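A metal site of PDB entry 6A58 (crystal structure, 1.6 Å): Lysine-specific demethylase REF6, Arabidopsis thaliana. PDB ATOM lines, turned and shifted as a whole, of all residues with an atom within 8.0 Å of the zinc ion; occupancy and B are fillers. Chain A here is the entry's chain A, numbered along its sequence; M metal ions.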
ATOM      1  N   VAL A 107     -15.317  11.398 -12.603  1.00  0.00           N
ATOM      2  CA  VAL A 107     -16.395  10.817 -11.819  1.00  0.00           C
ATOM      3  C   VAL A 107     -16.193  11.204 -10.352  1.00  0.00           C
ATOM      4  O   VAL A 107     -15.100  11.029  -9.821  1.00  0.00           O
ATOM      5  CB  VAL A 107     -16.427   9.273 -11.935  1.00  0.00           C
ATOM      6  CG1 VAL A 107     -17.657   8.693 -11.240  1.00  0.00           C
ATOM      7  CG2 VAL A 107     -16.386   8.856 -13.408  1.00  0.00           C
ATOM      8  N   CYS A 108     -17.248  11.725  -9.737  1.00  0.00           N
ATOM      9  CA  CYS A 108     -17.194  12.134  -8.328  1.00  0.00           C
ATOM     10  C   CYS A 108     -17.065  10.915  -7.428  1.00  0.00           C
ATOM     11  O   CYS A 108     -17.750   9.911  -7.628  1.00  0.00           O
ATOM     12  CB  CYS A 108     -18.441  12.936  -7.951  1.00  0.00           C
ATOM     13  SG  CYS A 108     -18.346  13.680  -6.317  1.00  0.00           S
ATOM     14  N   ALA A 109     -16.182  11.004  -6.431  1.00  0.00           N
ATOM     15  CA  ALA A 109     -15.860   9.880  -5.543  1.00  0.00           C
ATOM     16  C   ALA A 109     -16.757   9.764  -4.308  1.00  0.00           C
ATOM     17  O   ALA A 109     -16.627   8.787  -3.565  1.00  0.00           O
ATOM     18  CB  ALA A 109     -14.392   9.966  -5.121  1.00  0.00           C
ATOM     19  N   GLU A 110     -17.660  10.720  -4.084  1.00  0.00           N
ATOM     20  CA  GLU A 110     -18.586  10.681  -2.954  1.00  0.00           C
ATOM     21  C   GLU A 110     -19.588   9.533  -3.088  1.00  0.00           C
ATOM     22  O   GLU A 110     -19.948   9.167  -4.204  1.00  0.00           O
ATOM     23  CB  GLU A 110     -19.337  12.006  -2.816  1.00  0.00           C
ATOM     24  N   PRO A 111     -20.053   8.956  -1.948  1.00  0.00           N
ATOM     25  CA  PRO A 111     -20.810   7.700  -1.971  1.00  0.00           C
ATOM     26  C   PRO A 111     -22.203   7.795  -2.623  1.00  0.00           C
ATOM     27  O   PRO A 111     -22.572   6.906  -3.391  1.00  0.00           O
ATOM     28  CB  PRO A 111     -20.931   7.336  -0.481  1.00  0.00           C
ATOM     29  CG  PRO A 111     -20.843   8.637   0.239  1.00  0.00           C
ATOM     30  CD  PRO A 111     -19.983   9.540  -0.597  1.00  0.00           C
ATOM     31  N   ASP A 112     -22.941   8.867  -2.324  1.00  0.00           N
ATOM     32  CA  ASP A 112     -24.316   9.037  -2.826  1.00  0.00           C
ATOM     33  C   ASP A 112     -24.431  10.102  -3.935  1.00  0.00           C
ATOM     34  O   ASP A 112     -25.535  10.574  -4.207  1.00  0.00           O
ATOM     35  CB  ASP A 112     -25.242   9.411  -1.669  1.00  0.00           C
ATOM     36  N   CYS A 113     -23.318  10.452  -4.580  1.00  0.00           N
ATOM     37  CA  CYS A 113     -23.303  11.476  -5.622  1.00  0.00           C
ATOM     38  C   CYS A 113     -23.425  10.861  -7.016  1.00  0.00           C
ATOM     39  O   CYS A 113     -24.440  11.051  -7.684  1.00  0.00           O
ATOM     40  CB  CYS A 113     -22.038  12.342  -5.510  1.00  0.00           C
ATOM     41  SG  CYS A 113     -21.959  13.701  -6.708  1.00  0.00           S
ATOM     42  N   GLY A 114     -22.403  10.112  -7.432  1.00  0.00           N
ATOM     43  CA  GLY A 114     -22.390   9.465  -8.749  1.00  0.00           C
ATOM     44  C   GLY A 114     -22.318  10.370  -9.970  1.00  0.00           C
ATOM     45  O   GLY A 114     -22.535   9.914 -11.092  1.00  0.00           O
ATOM     46  N   GLN A 115     -21.989  11.642  -9.759  1.00  0.00           N
ATOM     47  CA  GLN A 115     -22.039  12.630 -10.833  1.00  0.00           C
ATOM     48  C   GLN A 115     -20.788  12.522 -11.713  1.00  0.00           C
ATOM     49  O   GLN A 115     -19.704  12.243 -11.195  1.00  0.00           O
ATOM     50  CB  GLN A 115     -22.169  14.041 -10.238  1.00  0.00           C
ATOM     51  CG  GLN A 115     -22.710  15.073 -11.204  1.00  0.00           C
ATOM     52  CD  GLN A 115     -23.281  16.317 -10.519  1.00  0.00           C
ATOM     53  OE1 GLN A 115     -23.641  16.301  -9.342  1.00  0.00           O
ATOM     54  NE2 GLN A 115     -23.374  17.389 -11.284  1.00  0.00           N
ATOM     55  N   THR A 116     -20.958  12.718 -13.024  1.00  0.00           N
ATOM     56  CA  THR A 116     -19.835  12.699 -13.967  1.00  0.00           C
ATOM     57  C   THR A 116     -19.720  14.020 -14.712  1.00  0.00           C
ATOM     58  O   THR A 116     -20.686  14.781 -14.815  1.00  0.00           O
ATOM     59  CB  THR A 116     -19.971  11.574 -15.013  1.00  0.00           C
ATOM     60  OG1 THR A 116     -21.061  11.889 -15.906  1.00  0.00           O
ATOM     61  CG2 THR A 116     -20.219  10.226 -14.345  1.00  0.00           C
ATOM     62  N   PHE A 117     -18.520  14.285 -15.247  1.00  0.00           N
ATOM     63  CA  PHE A 117     -18.197  15.556 -15.906  1.00  0.00           C
ATOM     64  C   PHE A 117     -17.352  15.316 -17.155  1.00  0.00           C
ATOM     65  O   PHE A 117     -16.564  14.373 -17.201  1.00  0.00           O
ATOM     66  CB  PHE A 117     -17.479  16.493 -14.926  1.00  0.00           C
ATOM     67  CG  PHE A 117     -18.233  16.672 -13.640  1.00  0.00           C
ATOM     68  CD1 PHE A 117     -19.215  17.647 -13.533  1.00  0.00           C
ATOM     69  CD2 PHE A 117     -18.022  15.798 -12.574  1.00  0.00           C
ATOM     70  CE1 PHE A 117     -19.944  17.786 -12.366  1.00  0.00           C
ATOM     71  CE2 PHE A 117     -18.751  15.937 -11.407  1.00  0.00           C
ATOM     72  CZ  PHE A 117     -19.716  16.933 -11.309  1.00  0.00           C
ATOM     73  N   PHE A 123     -15.594  19.538 -13.067  1.00  0.00           N
ATOM     74  CA  PHE A 123     -15.339  18.658 -11.926  1.00  0.00           C
ATOM     75  C   PHE A 123     -14.738  19.420 -10.737  1.00  0.00           C
ATOM     76  O   PHE A 123     -15.151  19.212  -9.598  1.00  0.00           O
ATOM     77  CB  PHE A 123     -14.443  17.474 -12.346  1.00  0.00           C
ATOM     78  CG  PHE A 123     -14.164  16.468 -11.253  1.00  0.00           C
ATOM     79  CD1 PHE A 123     -15.177  16.026 -10.397  1.00  0.00           C
ATOM     80  CD2 PHE A 123     -12.886  15.929 -11.103  1.00  0.00           C
ATOM     81  CE1 PHE A 123     -14.905  15.092  -9.402  1.00  0.00           C
ATOM     82  CE2 PHE A 123     -12.617  14.985 -10.116  1.00  0.00           C
ATOM     83  CZ  PHE A 123     -13.627  14.567  -9.266  1.00  0.00           C
ATOM     84  N   HIS A 126     -17.477  21.631  -9.241  1.00  0.00           N
ATOM     85  CA  HIS A 126     -18.370  20.774  -8.430  1.00  0.00           C
ATOM     86  C   HIS A 126     -17.771  20.475  -7.048  1.00  0.00           C
ATOM     87  O   HIS A 126     -18.477  20.561  -6.040  1.00  0.00           O
ATOM     88  CB  HIS A 126     -18.677  19.471  -9.174  1.00  0.00           C
ATOM     89  CG  HIS A 126     -19.465  18.478  -8.369  1.00  0.00           C
ATOM     90  ND1 HIS A 126     -20.817  18.618  -8.137  1.00  0.00           N
ATOM     91  CD2 HIS A 126     -19.098  17.327  -7.766  1.00  0.00           C
ATOM     92  CE1 HIS A 126     -21.245  17.602  -7.417  1.00  0.00           C
ATOM     93  NE2 HIS A 126     -20.220  16.801  -7.175  1.00  0.00           N
ATOM     94  N   LYS A 127     -16.489  20.115  -7.019  1.00  0.00           N
ATOM     95  CA  LYS A 127     -15.787  19.836  -5.757  1.00  0.00           C
ATOM     96  C   LYS A 127     -15.631  21.067  -4.859  1.00  0.00           C
ATOM     97  O   LYS A 127     -15.592  20.934  -3.636  1.00  0.00           O
ATOM     98  CB  LYS A 127     -14.409  19.201  -6.024  1.00  0.00           C
ATOM     99  CG  LYS A 127     -14.490  17.760  -6.507  1.00  0.00           C
ATOM    100  CD  LYS A 127     -13.127  17.111  -6.622  1.00  0.00           C
ATOM    101  CE  LYS A 127     -12.363  17.612  -7.839  1.00  0.00           C
ATOM    102  NZ  LYS A 127     -11.060  16.919  -8.022  1.00  0.00           N
ATOM    103  N   THR A 130     -19.740  22.020  -3.808  1.00  0.00           N
ATOM    104  CA  THR A 130     -20.114  21.031  -2.791  1.00  0.00           C
ATOM    105  C   THR A 130     -18.897  20.766  -1.898  1.00  0.00           C
ATOM    106  O   THR A 130     -17.881  21.445  -2.019  1.00  0.00           O
ATOM    107  CB  THR A 130     -20.610  19.719  -3.443  1.00  0.00           C
ATOM    108  OG1 THR A 130     -19.531  19.050  -4.114  1.00  0.00           O
ATOM    109  CG2 THR A 130     -21.728  20.003  -4.444  1.00  0.00           C
ATOM    110  N   GLY A 131     -19.021  19.803  -0.973  1.00  0.00           N
ATOM    111  CA  GLY A 131     -17.902  19.348  -0.156  1.00  0.00           C
ATOM    112  C   GLY A 131     -17.551  17.899  -0.466  1.00  0.00           C
ATOM    113  O   GLY A 131     -17.399  17.084   0.439  1.00  0.00           O
ATOM    114  N   HIS A 132     -17.419  17.603  -1.762  1.00  0.00           N
ATOM    115  CA  HIS A 132     -17.292  16.224  -2.260  1.00  0.00           C
ATOM    116  C   HIS A 132     -15.853  15.836  -2.573  1.00  0.00           C
ATOM    117  O   HIS A 132     -15.037  16.677  -2.962  1.00  0.00           O
ATOM    118  CB  HIS A 132     -18.159  16.046  -3.517  1.00  0.00           C
ATOM    119  CG  HIS A 132     -19.632  15.956  -3.222  1.00  0.00           C
ATOM    120  ND1 HIS A 132     -20.501  15.261  -4.030  1.00  0.00           N
ATOM    121  CD2 HIS A 132     -20.378  16.461  -2.208  1.00  0.00           C
ATOM    122  CE1 HIS A 132     -21.720  15.349  -3.537  1.00  0.00           C
ATOM    123  NE2 HIS A 132     -21.674  16.066  -2.430  1.00  0.00           N
ATOM    124  N   SER A 133     -15.567  14.545  -2.437  1.00  0.00           N
ATOM    125  CA  SER A 133     -14.247  13.991  -2.737  1.00  0.00           C
ATOM    126  C   SER A 133     -14.055  13.841  -4.239  1.00  0.00           C
ATOM    127  O   SER A 133     -14.948  13.366  -4.953  1.00  0.00           O
ATOM    128  CB  SER A 133     -14.073  12.630  -2.050  1.00  0.00           C
ATOM    129  OG  SER A 133     -12.764  12.114  -2.233  1.00  0.00           O
HETATM  130 ZN    ZN M   1     -20.055  14.898  -6.185  1.00  0.00          ZN
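O of His 126 sits at hydrogen-bond distance from OG1 of Thr 130, 2.7 Å away.
The backbone NH (N) of Glu 110 sits close to the side-chain sulfur (SG) of Cys 108 (3.8 Å).
N of His 132 sits close to OG1 of Thr 130, 3.5 Å away.
The side-chain sulfur (SG) of Cys 113 lies close to the backbone NH (N) of Gln 115.
SG of Cys 108 lies close to O of Ser 133 (3.7 Å).
N of Cys 108 lies within hydrogen-bond range of O of Gln 115 (2.9 Å).
SG of Cys 108 is bound to the zinc ion, 2.1 Å away.
The zinc ion is bound by NE2 of His 126, at 2.2 Å.
The zinc ion is bound by ND1 of His 132 (2.2 Å).
SG of Cys 113 is bound to the zinc ion (2.3 Å).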
